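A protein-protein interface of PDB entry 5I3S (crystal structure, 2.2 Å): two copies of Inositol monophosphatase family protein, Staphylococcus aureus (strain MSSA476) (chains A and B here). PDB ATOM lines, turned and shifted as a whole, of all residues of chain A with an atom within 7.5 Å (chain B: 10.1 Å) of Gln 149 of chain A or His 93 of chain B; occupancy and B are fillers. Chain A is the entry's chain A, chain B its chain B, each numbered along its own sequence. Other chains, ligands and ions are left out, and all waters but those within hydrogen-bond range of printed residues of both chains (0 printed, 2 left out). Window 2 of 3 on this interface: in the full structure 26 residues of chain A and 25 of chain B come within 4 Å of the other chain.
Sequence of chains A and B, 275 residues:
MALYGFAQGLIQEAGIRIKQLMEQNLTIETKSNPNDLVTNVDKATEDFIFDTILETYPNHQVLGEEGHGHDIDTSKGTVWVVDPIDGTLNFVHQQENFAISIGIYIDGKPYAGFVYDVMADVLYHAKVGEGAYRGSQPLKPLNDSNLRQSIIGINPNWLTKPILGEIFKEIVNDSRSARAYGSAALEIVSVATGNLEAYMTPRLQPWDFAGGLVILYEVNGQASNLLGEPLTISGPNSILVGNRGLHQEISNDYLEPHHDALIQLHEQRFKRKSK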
ATOM      1  N   SER A 145     -17.536   0.801   5.782  1.00  0.00           N
ATOM      2  CA  SER A 145     -16.897  -0.332   5.124  1.00  0.00           C
ATOM      3  C   SER A 145     -16.060   0.192   3.971  1.00  0.00           C
ATOM      4  O   SER A 145     -16.321   1.287   3.429  1.00  0.00           O
ATOM      5  CB  SER A 145     -17.981  -1.330   4.608  1.00  0.00           C
ATOM      6  OG  SER A 145     -18.772  -0.739   3.577  1.00  0.00           O
ATOM      7  N   ASN A 146     -15.063  -0.595   3.586  1.00  0.00           N
ATOM      8  CA  ASN A 146     -14.429  -0.416   2.265  1.00  0.00           C
ATOM      9  C   ASN A 146     -15.201  -1.149   1.159  1.00  0.00           C
ATOM     10  O   ASN A 146     -15.812  -2.215   1.412  1.00  0.00           O
ATOM     11  CB  ASN A 146     -12.960  -0.871   2.323  1.00  0.00           C
ATOM     12  CG  ASN A 146     -12.188  -0.116   3.411  1.00  0.00           C
ATOM     13  OD1 ASN A 146     -12.102   1.100   3.369  1.00  0.00           O
ATOM     14  ND2 ASN A 146     -11.683  -0.841   4.421  1.00  0.00           N
ATOM     15  N   LEU A 147     -15.150  -0.608  -0.058  1.00  0.00           N
ATOM     16  CA  LEU A 147     -15.860  -1.207  -1.199  1.00  0.00           C
ATOM     17  C   LEU A 147     -15.442  -2.669  -1.421  1.00  0.00           C
ATOM     18  O   LEU A 147     -16.309  -3.561  -1.664  1.00  0.00           O
ATOM     19  CB  LEU A 147     -15.651  -0.401  -2.499  1.00  0.00           C
ATOM     20  CG  LEU A 147     -16.409  -0.962  -3.712  1.00  0.00           C
ATOM     21  CD1 LEU A 147     -17.924  -0.979  -3.535  1.00  0.00           C
ATOM     22  CD2 LEU A 147     -16.087  -0.132  -4.918  1.00  0.00           C
ATOM     23  N   ARG A 148     -14.137  -2.912  -1.277  1.00  0.00           N
ATOM     24  CA  ARG A 148     -13.504  -4.247  -1.429  1.00  0.00           C
ATOM     25  C   ARG A 148     -14.097  -5.349  -0.520  1.00  0.00           C
ATOM     26  O   ARG A 148     -13.983  -6.503  -0.837  1.00  0.00           O
ATOM     27  CB  ARG A 148     -11.977  -4.121  -1.168  1.00  0.00           C
ATOM     28  N   GLN A 149     -14.657  -4.980   0.629  1.00  0.00           N
ATOM     29  CA  GLN A 149     -15.387  -5.896   1.512  1.00  0.00           C
ATOM     30  C   GLN A 149     -16.891  -5.638   1.554  1.00  0.00           C
ATOM     31  O   GLN A 149     -17.560  -6.088   2.457  1.00  0.00           O
ATOM     32  CB  GLN A 149     -14.854  -5.771   2.967  1.00  0.00           C
ATOM     33  CG  GLN A 149     -13.642  -6.641   3.257  1.00  0.00           C
ATOM     34  CD  GLN A 149     -12.347  -5.862   3.138  1.00  0.00           C
ATOM     35  OE1 GLN A 149     -12.161  -4.830   3.814  1.00  0.00           O
ATOM     36  NE2 GLN A 149     -11.438  -6.335   2.271  1.00  0.00           N
ATOM     37  N   SER A 150     -17.430  -4.881   0.618  1.00  0.00           N
ATOM     38  CA  SER A 150     -18.866  -4.553   0.651  1.00  0.00           C
ATOM     39  C   SER A 150     -19.608  -5.350  -0.425  1.00  0.00           C
ATOM     40  O   SER A 150     -19.033  -5.686  -1.463  1.00  0.00           O
ATOM     41  CB  SER A 150     -19.073  -3.054   0.431  1.00  0.00           C
ATOM     42  OG  SER A 150     -18.282  -2.307   1.329  1.00  0.00           O
ATOM     43  N   ILE A 151     -20.865  -5.658  -0.133  1.00  0.00           N
ATOM     44  CA  ILE A 151     -21.884  -6.096  -1.098  1.00  0.00           C
ATOM     45  C   ILE A 151     -22.761  -4.924  -1.430  1.00  0.00           C
ATOM     46  O   ILE A 151     -23.230  -4.246  -0.520  1.00  0.00           O
ATOM     47  CB  ILE A 151     -22.857  -7.109  -0.462  1.00  0.00           C
ATOM     48  CG1 ILE A 151     -22.096  -8.281   0.175  1.00  0.00           C
ATOM     49  CG2 ILE A 151     -23.819  -7.654  -1.516  1.00  0.00           C
ATOM     50  CD1 ILE A 151     -23.053  -9.302   0.787  1.00  0.00           C
ATOM     51  N   ASP A 174     -14.757  -3.973  -8.132  1.00  0.00           N
ATOM     52  CA  ASP A 174     -14.035  -3.866  -6.882  1.00  0.00           C
ATOM     53  C   ASP A 174     -14.854  -4.405  -5.724  1.00  0.00           C
ATOM     54  O   ASP A 174     -14.281  -4.987  -4.813  1.00  0.00           O
ATOM     55  CB  ASP A 174     -13.487  -2.456  -6.677  1.00  0.00           C
ATOM     56  CG  ASP A 174     -12.373  -2.144  -7.707  1.00  0.00           C
ATOM     57  OD1 ASP A 174     -11.412  -2.960  -7.861  1.00  0.00           O
ATOM     58  OD2 ASP A 174     -12.454  -1.114  -8.399  1.00  0.00           O
ATOM     59  N   SER A 175     -16.177  -4.273  -5.770  1.00  0.00           N
ATOM     60  CA  SER A 175     -16.986  -4.814  -4.669  1.00  0.00           C
ATOM     61  C   SER A 175     -16.773  -6.328  -4.548  1.00  0.00           C
ATOM     62  O   SER A 175     -16.282  -7.014  -5.468  1.00  0.00           O
ATOM     63  CB  SER A 175     -18.461  -4.469  -4.797  1.00  0.00           C
ATOM     64  OG  SER A 175     -18.886  -4.584  -6.127  1.00  0.00           O
ATOM     65  N   ARG A 176     -17.065  -6.817  -3.364  1.00  0.00           N
ATOM     66  CA  ARG A 176     -16.921  -8.232  -3.060  1.00  0.00           C
ATOM     67  C   ARG A 176     -17.967  -9.021  -3.805  1.00  0.00           C
ATOM     68  O   ARG A 176     -17.666 -10.099  -4.349  1.00  0.00           O
ATOM     69  CB  ARG A 176     -17.082  -8.450  -1.564  1.00  0.00           C
ATOM     70  CG  ARG A 176     -16.677  -9.814  -1.083  1.00  0.00           C
ATOM     71  CD  ARG A 176     -15.167 -10.046  -1.150  1.00  0.00           C
ATOM     72  NE  ARG A 176     -14.856 -11.371  -0.633  1.00  0.00           N
ATOM     73  CZ  ARG A 176     -15.053 -12.522  -1.297  1.00  0.00           C
ATOM     74  NH1 ARG A 176     -15.546 -12.552  -2.546  1.00  0.00           N
ATOM     75  NH2 ARG A 176     -14.749 -13.676  -0.692  1.00  0.00           N
ATOM     76  N   SER A 177     -19.208  -8.518  -3.785  1.00  0.00           N
ATOM     77  CA  SER A 177     -20.242  -9.051  -4.668  1.00  0.00           C
ATOM     78  C   SER A 177     -21.410  -8.085  -4.864  1.00  0.00           C
ATOM     79  O   SER A 177     -21.418  -6.966  -4.319  1.00  0.00           O
ATOM     80  CB  SER A 177     -20.765 -10.429  -4.180  1.00  0.00           C
ATOM     81  OG  SER A 177     -21.655 -10.987  -5.147  1.00  0.00           O
ATOM     82  N   ARG A 179     -25.890  -7.737  -5.640  1.00  0.00           N
ATOM     83  CA  ARG A 179     -27.232  -8.219  -5.383  1.00  0.00           C
ATOM     84  C   ARG A 179     -28.221  -7.270  -6.065  1.00  0.00           C
ATOM     85  O   ARG A 179     -27.879  -6.147  -6.382  1.00  0.00           O
ATOM     86  CB  ARG A 179     -27.513  -8.219  -3.866  1.00  0.00           C
ATOM     87  CG  ARG A 179     -26.550  -9.017  -3.021  1.00  0.00           C
ATOM     88  CD  ARG A 179     -26.742 -10.524  -3.253  1.00  0.00           C
ATOM     89  NE  ARG A 179     -25.854 -11.324  -2.418  1.00  0.00           N
ATOM     90  CZ  ARG A 179     -24.636 -11.732  -2.743  1.00  0.00           C
ATOM     91  NH1 ARG A 179     -24.078 -11.451  -3.939  1.00  0.00           N
ATOM     92  NH2 ARG A 179     -23.962 -12.475  -1.873  1.00  0.00           N
ATOM     93  N   SER A 190     -32.540  -2.124   3.077  1.00  0.00           N
ATOM     94  CA  SER A 190     -31.418  -3.056   3.219  1.00  0.00           C
ATOM     95  C   SER A 190     -30.119  -2.343   3.522  1.00  0.00           C
ATOM     96  O   SER A 190     -29.257  -2.884   4.227  1.00  0.00           O
ATOM     97  CB  SER A 190     -31.202  -3.875   1.967  1.00  0.00           C
ATOM     98  OG  SER A 190     -32.319  -4.664   1.683  1.00  0.00           O
ATOM     99  N   THR A 193     -30.521  -1.402   7.304  1.00  0.00           N
ATOM    100  CA  THR A 193     -30.352  -2.552   8.199  1.00  0.00           C
ATOM    101  C   THR A 193     -28.981  -3.175   8.150  1.00  0.00           C
ATOM    102  O   THR A 193     -28.705  -4.061   8.944  1.00  0.00           O
ATOM    103  CB  THR A 193     -31.368  -3.698   7.904  1.00  0.00           C
ATOM    104  OG1 THR A 193     -31.235  -4.137   6.548  1.00  0.00           O
ATOM    105  CG2 THR A 193     -32.827  -3.229   8.146  1.00  0.00           C
ATOM    106  N   GLY A 194     -28.132  -2.775   7.212  1.00  0.00           N
ATOM    107  CA  GLY A 194     -26.817  -3.393   7.060  1.00  0.00           C
ATOM    108  C   GLY A 194     -26.768  -4.630   6.195  1.00  0.00           C
ATOM    109  O   GLY A 194     -25.712  -5.233   6.076  1.00  0.00           O
ATOM    110  N   ASN A 195     -27.885  -5.002   5.555  1.00  0.00           N
ATOM    111  CA  ASN A 195     -27.896  -6.132   4.634  1.00  0.00           C
ATOM    112  C   ASN A 195     -27.161  -5.872   3.309  1.00  0.00           C
ATOM    113  O   ASN A 195     -26.675  -6.818   2.667  1.00  0.00           O
ATOM    114  CB  ASN A 195     -29.333  -6.617   4.372  1.00  0.00           C
ATOM    115  CG  ASN A 195     -29.770  -7.678   5.370  1.00  0.00           C
ATOM    116  OD1 ASN A 195     -29.155  -7.849   6.462  1.00  0.00           O
ATOM    117  ND2 ASN A 195     -30.828  -8.419   5.016  1.00  0.00           N
ATOM    118  N   LEU A 196     -27.102  -4.612   2.902  1.00  0.00           N
ATOM    119  CA  LEU A 196     -26.270  -4.172   1.805  1.00  0.00           C
ATOM    120  C   LEU A 196     -25.488  -2.954   2.299  1.00  0.00           C
ATOM    121  O   LEU A 196     -26.031  -2.145   3.050  1.00  0.00           O
ATOM    122  CB  LEU A 196     -27.131  -3.740   0.618  1.00  0.00           C
ATOM    123  CG  LEU A 196     -28.049  -4.716  -0.125  1.00  0.00           C
ATOM    124  CD1 LEU A 196     -28.834  -3.986  -1.222  1.00  0.00           C
ATOM    125  CD2 LEU A 196     -27.206  -5.836  -0.716  1.00  0.00           C
ATOM    126  N   GLU A 197     -24.250  -2.805   1.849  1.00  0.00           N
ATOM    127  CA  GLU A 197     -23.433  -1.674   2.219  1.00  0.00           C
ATOM    128  C   GLU A 197     -23.706  -0.532   1.312  1.00  0.00           C
ATOM    129  O   GLU A 197     -23.572   0.607   1.739  1.00  0.00           O
ATOM    130  CB  GLU A 197     -21.921  -1.991   2.225  1.00  0.00           C
ATOM    131  CG  GLU A 197     -21.419  -2.762   3.453  1.00  0.00           C
ATOM    132  CD  GLU A 197     -21.633  -4.266   3.425  1.00  0.00           C
ATOM    133  OE1 GLU A 197     -22.073  -4.860   2.415  1.00  0.00           O
ATOM    134  OE2 GLU A 197     -21.304  -4.895   4.437  1.00  0.00           O
ATOM    135  N   LEU A 246     -18.248   4.150   2.542  1.00  0.00           N
ATOM    136  CA  LEU A 246     -18.086   3.715   1.226  1.00  0.00           C
ATOM    137  C   LEU A 246     -18.954   4.445   0.228  1.00  0.00           C
ATOM    138  O   LEU A 246     -18.706   4.352  -0.979  1.00  0.00           O
ATOM    139  CB  LEU A 246     -18.233   2.258   1.177  1.00  0.00           C
ATOM    140  CG  LEU A 246     -19.367   1.807   0.372  1.00  0.00           C
ATOM    141  CD1 LEU A 246     -18.886   0.459  -0.106  1.00  0.00           C
ATOM    142  CD2 LEU A 246     -20.585   1.928   1.300  1.00  0.00           C
ATOM    143  N   GLU A 249     -16.096   6.682  -0.805  1.00  0.00           N
ATOM    144  CA  GLU A 249     -15.210   5.947  -1.756  1.00  0.00           C
ATOM    145  C   GLU A 249     -15.840   5.722  -3.151  1.00  0.00           C
ATOM    146  O   GLU A 249     -15.164   5.876  -4.182  1.00  0.00           O
ATOM    147  CB  GLU A 249     -14.812   4.587  -1.152  1.00  0.00           C
ATOM    148  CG  GLU A 249     -13.810   3.724  -1.951  1.00  0.00           C
ATOM    149  CD  GLU A 249     -13.584   2.386  -1.322  1.00  0.00           C
ATOM    150  OE1 GLU A 249     -14.201   2.059  -0.256  1.00  0.00           O
ATOM    151  OE2 GLU A 249     -12.822   1.585  -1.929  1.00  0.00           O
ATOM    152  N   MET B  22     -23.928 -19.323  15.662  1.00  0.00           N
ATOM    153  CA  MET B  22     -24.120 -17.891  15.477  1.00  0.00           C
ATOM    154  C   MET B  22     -24.518 -17.306  16.827  1.00  0.00           C
ATOM    155  O   MET B  22     -23.976 -16.292  17.242  1.00  0.00           O
ATOM    156  CB  MET B  22     -25.235 -17.611  14.462  1.00  0.00           C
ATOM    157  CG  MET B  22     -24.973 -18.102  13.028  1.00  0.00           C
ATOM    158  SD  MET B  22     -26.457 -18.149  11.994  1.00  0.00           S
ATOM    159  CE  MET B  22     -26.487 -16.409  11.587  1.00  0.00           C
ATOM    160  N   ASN B  35     -15.954 -13.114  10.264  1.00  0.00           N
ATOM    161  CA  ASN B  35     -15.479 -13.829   9.096  1.00  0.00           C
ATOM    162  C   ASN B  35     -14.664 -15.104   9.379  1.00  0.00           C
ATOM    163  O   ASN B  35     -14.488 -15.957   8.488  1.00  0.00           O
ATOM    164  CB  ASN B  35     -14.654 -12.896   8.229  1.00  0.00           C
ATOM    165  CG  ASN B  35     -14.947 -13.088   6.749  1.00  0.00           C
ATOM    166  OD1 ASN B  35     -15.403 -12.160   6.066  1.00  0.00           O
ATOM    167  ND2 ASN B  35     -14.730 -14.310   6.259  1.00  0.00           N
ATOM    168  N   LEU B  37     -16.000 -16.798  11.802  1.00  0.00           N
ATOM    169  CA  LEU B  37     -17.213 -17.487  12.165  1.00  0.00           C
ATOM    170  C   LEU B  37     -17.653 -18.376  10.997  1.00  0.00           C
ATOM    171  O   LEU B  37     -17.770 -19.577  11.158  1.00  0.00           O
ATOM    172  CB  LEU B  37     -18.304 -16.480  12.517  1.00  0.00           C
ATOM    173  CG  LEU B  37     -19.619 -17.055  13.077  1.00  0.00           C
ATOM    174  CD1 LEU B  37     -19.314 -17.898  14.315  1.00  0.00           C
ATOM    175  CD2 LEU B  37     -20.666 -15.972  13.366  1.00  0.00           C
ATOM    176  N   VAL B  38     -17.805 -17.801   9.807  1.00  0.00           N
ATOM    177  CA  VAL B  38     -18.258 -18.560   8.650  1.00  0.00           C
ATOM    178  C   VAL B  38     -17.344 -19.751   8.365  1.00  0.00           C
ATOM    179  O   VAL B  38     -17.840 -20.850   8.097  1.00  0.00           O
ATOM    180  CB  VAL B  38     -18.507 -17.654   7.396  1.00  0.00           C
ATOM    181  CG1 VAL B  38     -17.216 -17.181   6.772  1.00  0.00           C
ATOM    182  CG2 VAL B  38     -19.352 -18.369   6.358  1.00  0.00           C
ATOM    183  N   ILE B  85     -22.886 -24.268   3.850  1.00  0.00           N
ATOM    184  CA  ILE B  85     -23.320 -22.881   3.744  1.00  0.00           C
ATOM    185  C   ILE B  85     -23.226 -22.440   2.281  1.00  0.00           C
ATOM    186  O   ILE B  85     -22.136 -22.051   1.813  1.00  0.00           O
ATOM    187  CB  ILE B  85     -22.466 -21.944   4.629  1.00  0.00           C
ATOM    188  CG1 ILE B  85     -22.526 -22.409   6.088  1.00  0.00           C
ATOM    189  CG2 ILE B  85     -23.010 -20.514   4.521  1.00  0.00           C
ATOM    190  CD1 ILE B  85     -21.702 -21.581   7.062  1.00  0.00           C
ATOM    191  N   GLY B  87     -23.981 -19.628   0.181  1.00  0.00           N
ATOM    192  CA  GLY B  87     -24.168 -18.192   0.256  1.00  0.00           C
ATOM    193  C   GLY B  87     -23.350 -17.678   1.428  1.00  0.00           C
ATOM    194  O   GLY B  87     -23.908 -17.112   2.384  1.00  0.00           O
ATOM    195  N   THR B  88     -22.033 -17.872   1.373  1.00  0.00           N
ATOM    196  CA  THR B  88     -21.199 -17.595   2.522  1.00  0.00           C
ATOM    197  C   THR B  88     -21.114 -16.117   2.732  1.00  0.00           C
ATOM    198  O   THR B  88     -21.045 -15.675   3.894  1.00  0.00           O
ATOM    199  CB  THR B  88     -19.791 -18.173   2.369  1.00  0.00           C
ATOM    200  OG1 THR B  88     -19.305 -17.827   1.084  1.00  0.00           O
ATOM    201  CG2 THR B  88     -19.801 -19.708   2.542  1.00  0.00           C
ATOM    202  N   LEU B  89     -21.109 -15.348   1.636  1.00  0.00           N
ATOM    203  CA  LEU B  89     -21.139 -13.876   1.746  1.00  0.00           C
ATOM    204  C   LEU B  89     -22.410 -13.362   2.378  1.00  0.00           C
ATOM    205  O   LEU B  89     -22.369 -12.389   3.167  1.00  0.00           O
ATOM    206  CB  LEU B  89     -20.971 -13.155   0.395  1.00  0.00           C
ATOM    207  CG  LEU B  89     -19.515 -12.972   0.001  1.00  0.00           C
ATOM    208  CD1 LEU B  89     -19.469 -12.286  -1.367  1.00  0.00           C
ATOM    209  CD2 LEU B  89     -18.733 -12.168   1.066  1.00  0.00           C
ATOM    210  N   ASN B  90     -23.543 -13.959   2.012  1.00  0.00           N
ATOM    211  CA  ASN B  90     -24.807 -13.583   2.700  1.00  0.00           C
ATOM    212  C   ASN B  90     -24.760 -13.844   4.213  1.00  0.00           C
ATOM    213  O   ASN B  90     -25.333 -13.070   4.982  1.00  0.00           O
ATOM    214  CB  ASN B  90     -26.013 -14.285   2.083  1.00  0.00           C
ATOM    215  CG  ASN B  90     -26.322 -13.785   0.701  1.00  0.00           C
ATOM    216  OD1 ASN B  90     -25.769 -12.770   0.246  1.00  0.00           O
ATOM    217  ND2 ASN B  90     -27.198 -14.493   0.011  1.00  0.00           N
ATOM    218  N   PHE B  91     -24.089 -14.928   4.610  1.00  0.00           N
ATOM    219  CA  PHE B  91     -23.962 -15.311   6.024  1.00  0.00           C
ATOM    220  C   PHE B  91     -23.174 -14.232   6.780  1.00  0.00           C
ATOM    221  O   PHE B  91     -23.639 -13.691   7.757  1.00  0.00           O
ATOM    222  CB  PHE B  91     -23.295 -16.689   6.117  1.00  0.00           C
ATOM    223  CG  PHE B  91     -23.023 -17.154   7.524  1.00  0.00           C
ATOM    224  CD1 PHE B  91     -23.759 -18.186   8.087  1.00  0.00           C
ATOM    225  CD2 PHE B  91     -21.969 -16.595   8.271  1.00  0.00           C
ATOM    226  CE1 PHE B  91     -23.482 -18.616   9.391  1.00  0.00           C
ATOM    227  CE2 PHE B  91     -21.688 -17.032   9.559  1.00  0.00           C
ATOM    228  CZ  PHE B  91     -22.433 -18.031  10.118  1.00  0.00           C
ATOM    229  N   VAL B  92     -22.012 -13.888   6.252  1.00  0.00           N
ATOM    230  CA  VAL B  92     -21.168 -12.885   6.829  1.00  0.00           C
ATOM    231  C   VAL B  92     -21.907 -11.544   6.939  1.00  0.00           C
ATOM    232  O   VAL B  92     -21.903 -10.962   8.027  1.00  0.00           O
ATOM    233  CB  VAL B  92     -19.844 -12.775   6.050  1.00  0.00           C
ATOM    234  CG1 VAL B  92     -18.981 -11.611   6.529  1.00  0.00           C
ATOM    235  CG2 VAL B  92     -19.015 -14.044   6.222  1.00  0.00           C
ATOM    236  N   HIS B  93     -22.547 -11.077   5.838  1.00  0.00           N
ATOM    237  CA  HIS B  93     -23.026  -9.668   5.738  1.00  0.00           C
ATOM    238  C   HIS B  93     -24.476  -9.479   6.133  1.00  0.00           C
ATOM    239  O   HIS B  93     -24.878  -8.409   6.522  1.00  0.00           O
ATOM    240  CB  HIS B  93     -22.809  -9.118   4.325  1.00  0.00           C
ATOM    241  CG  HIS B  93     -21.362  -8.895   4.002  1.00  0.00           C
ATOM    242  ND1 HIS B  93     -20.756  -7.670   4.137  1.00  0.00           N
ATOM    243  CD2 HIS B  93     -20.384  -9.751   3.634  1.00  0.00           C
ATOM    244  CE1 HIS B  93     -19.479  -7.770   3.812  1.00  0.00           C
ATOM    245  NE2 HIS B  93     -19.228  -9.022   3.496  1.00  0.00           N
ATOM    246  N   GLN B  94     -25.270 -10.527   5.999  1.00  0.00           N
ATOM    247  CA  GLN B  94     -26.678 -10.418   6.216  1.00  0.00           C
ATOM    248  C   GLN B  94     -27.183 -11.319   7.353  1.00  0.00           C
ATOM    249  O   GLN B  94     -28.280 -11.102   7.829  1.00  0.00           O
ATOM    250  CB  GLN B  94     -27.398 -10.693   4.917  1.00  0.00           C
ATOM    251  CG  GLN B  94     -26.865  -9.962   3.687  1.00  0.00           C
ATOM    252  CD  GLN B  94     -27.783 -10.121   2.449  1.00  0.00           C
ATOM    253  OE1 GLN B  94     -28.357 -11.162   2.250  1.00  0.00           O
ATOM    254  NE2 GLN B  94     -27.922  -9.084   1.644  1.00  0.00           N
ATOM    255  N   GLN B  95     -26.395 -12.318   7.785  1.00  0.00           N
ATOM    256  CA  GLN B  95     -26.823 -13.294   8.823  1.00  0.00           C
ATOM    257  C   GLN B  95     -28.077 -14.053   8.402  1.00  0.00           C
ATOM    258  O   GLN B  95     -28.835 -14.449   9.259  1.00  0.00           O
ATOM    259  CB  GLN B  95     -27.112 -12.592  10.196  1.00  0.00           C
ATOM    260  CG  GLN B  95     -25.926 -11.925  10.848  1.00  0.00           C
ATOM    261  CD  GLN B  95     -25.607 -10.524  10.312  1.00  0.00           C
ATOM    262  OE1 GLN B  95     -26.427  -9.584  10.362  1.00  0.00           O
ATOM    263  NE2 GLN B  95     -24.388 -10.376   9.830  1.00  0.00           N
ATOM    264  N   GLU B  96     -28.297 -14.205   7.100  1.00  0.00           N
ATOM    265  CA  GLU B  96     -29.509 -14.780   6.503  1.00  0.00           C
ATOM    266  C   GLU B  96     -29.308 -14.917   4.978  1.00  0.00           C
ATOM    267  O   GLU B  96     -28.225 -14.599   4.465  1.00  0.00           O
ATOM    268  CB  GLU B  96     -30.780 -13.983   6.854  1.00  0.00           C
ATOM    269  CG  GLU B  96     -30.914 -12.612   6.209  1.00  0.00           C
ATOM    270  CD  GLU B  96     -32.170 -11.834   6.613  1.00  0.00           C
ATOM    271  OE1 GLU B  96     -32.217 -10.621   6.367  1.00  0.00           O
ATOM    272  OE2 GLU B  96     -33.124 -12.418   7.150  1.00  0.00           O
ATOM    273  N   ASN B  97     -30.304 -15.455   4.267  1.00  0.00           N
ATOM    274  CA  ASN B  97     -30.234 -15.706   2.794  1.00  0.00           C
ATOM    275  C   ASN B  97     -29.141 -16.715   2.390  1.00  0.00           C
ATOM    276  O   ASN B  97     -28.551 -16.615   1.321  1.00  0.00           O
ATOM    277  CB  ASN B  97     -30.160 -14.380   2.027  1.00  0.00           C
ATOM    278  CG  ASN B  97     -31.236 -13.398   2.494  1.00  0.00           C
ATOM    279  OD1 ASN B  97     -32.330 -13.827   2.843  1.00  0.00           O
ATOM    280  ND2 ASN B  97     -30.944 -12.083   2.500  1.00  0.00           N
ATOM    281  N   PHE B  98     -28.881 -17.691   3.266  1.00  0.00           N
ATOM    282  CA  PHE B  98     -27.935 -18.798   2.996  1.00  0.00           C
ATOM    283  C   PHE B  98     -28.610 -20.125   3.258  1.00  0.00           C
ATOM    284  O   PHE B  98     -29.564 -20.199   4.004  1.00  0.00           O
ATOM    285  CB  PHE B  98     -26.662 -18.690   3.837  1.00  0.00           C
ATOM    286  CG  PHE B  98     -26.881 -18.796   5.351  1.00  0.00           C
ATOM    287  CD1 PHE B  98     -26.881 -20.053   5.996  1.00  0.00           C
ATOM    288  CD2 PHE B  98     -27.053 -17.658   6.131  1.00  0.00           C
ATOM    289  CE1 PHE B  98     -27.070 -20.138   7.387  1.00  0.00           C
ATOM    290  CE2 PHE B  98     -27.257 -17.760   7.517  1.00  0.00           C
ATOM    291  CZ  PHE B  98     -27.263 -18.996   8.145  1.00  0.00           C
ATOM    292  N   TYR B 181     -29.566 -12.949  -5.758  1.00  0.00           N
ATOM    293  CA  TYR B 181     -29.716 -13.216  -4.306  1.00  0.00           C
ATOM    294  C   TYR B 181     -28.472 -13.768  -3.655  1.00  0.00           C
ATOM    295  O   TYR B 181     -28.390 -13.781  -2.443  1.00  0.00           O
ATOM    296  CB  TYR B 181     -30.904 -14.157  -4.035  1.00  0.00           C
ATOM    297  CG  TYR B 181     -32.166 -13.709  -4.698  1.00  0.00           C
ATOM    298  CD1 TYR B 181     -32.693 -12.461  -4.442  1.00  0.00           C
ATOM    299  CD2 TYR B 181     -32.839 -14.505  -5.571  1.00  0.00           C
ATOM    300  CE1 TYR B 181     -33.863 -12.031  -5.062  1.00  0.00           C
ATOM    301  CE2 TYR B 181     -34.004 -14.083  -6.183  1.00  0.00           C
ATOM    302  CZ  TYR B 181     -34.493 -12.839  -5.924  1.00  0.00           C
ATOM    303  OH  TYR B 181     -35.656 -12.413  -6.488  1.00  0.00           O
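N of Arg 176 of chain A is in hydrogen-bond range of O of Ser 150 of chain A (3.0 Å). The guanidinium group (NH1) of Arg 179 of chain A sits at hydrogen-bond distance from the side-chain hydroxyl (OG) of Ser 177 of chain A. The side-chain amide nitrogen (ND2) of Asn 90 of chain B is in hydrogen-bond range of the backbone carbonyl oxygen (O) of Tyr 181 of chain B (2.8 Å). OE1 of Gln 94 of chain B is in hydrogen-bond range of ND2 of Asn 97 of chain B, 2.8 Å away.
Among the printed residues, merely in contact across the chains: Gln 149 of chain A with His 93 of chain B, Arg 179 of chain A with Tyr 181 of chain B, Ile 151 of chain A with His 93 of chain B, Ser 177 of chain A with Leu 89 of chain B, Arg 176 of chain A with Leu 89 of chain B, Arg 179 of chain A with Leu 89 of chain B and Ile 151 of chain A with Leu 89 of chain B.
The guanidinium group (NH2) of Arg 179 of chain A sits at hydrogen-bond distance from the side-chain amide oxygen (OD1) of Asn 90 of chain B (2.8 Å). O of Asn 195 of chain A lies within hydrogen-bond range of NE2 of Gln 94 of chain B (2.8 Å). The side-chain amide nitrogen (ND2) of Asn 195 of chain A lies within hydrogen-bond range of the side-chain carboxylate (OE1) of Glu 96 of chain B. ND1 of His 93 of chain B lies within hydrogen-bond range of OE2 of Glu 197 of chain A. The backbone carbonyl oxygen (O) of Gly 194 of chain A lies close to the backbone carbonyl oxygen (O) of His 93 of chain B, at 3.3 Å.
No position is printed for both chains. Of the 12 pairs that touch across the chains among the printed residues, none has its exchanged pair printed and touching as well.
Asn 146 of chain A touches none of the printed residues of chain B. No residue of chain B comes within 4 Å of Arg 148 of chain A. Of the printed residues of chain B, Gln 149 of chain A touches His 93 (2.9 Å). Of the printed residues of chain B, Asn 195 of chain A touches Gln 94 and Glu 96. Glu 249 of chain A touches none of the printed residues of chain B. Of the printed residues of chain A, Asn 90 of chain B touches Arg 179 (2.8 Å). His 93 of chain B touches just these residues of chain A: Gln 149, Ile 151, Gly 194 and Glu 197. Of the printed residues of chain A, Gln 94 of chain B touches Asn 195. Printed residues of chain A within 4 Å of Tyr 181 of chain B: Arg 179 (3.5 Å). The nearest residue of chain A that does not touch His 93 of chain B is Asn 195 of chain A (4.2 Å).
Hydrophobic or aromatic side chains of chain A within 4 Å of the printed part of chain B: Ile 151. Of the 18 printed residues of chain B, 6 touch a printed residue of chain A. Hydrophobic or aromatic side chains of chain B that line the printed part of chain A: Leu 89 and His 93. Among the printed residues, no Asp or Glu carboxylate lies within 4 Å of a Lys or Arg side-chain nitrogen of the other chain.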
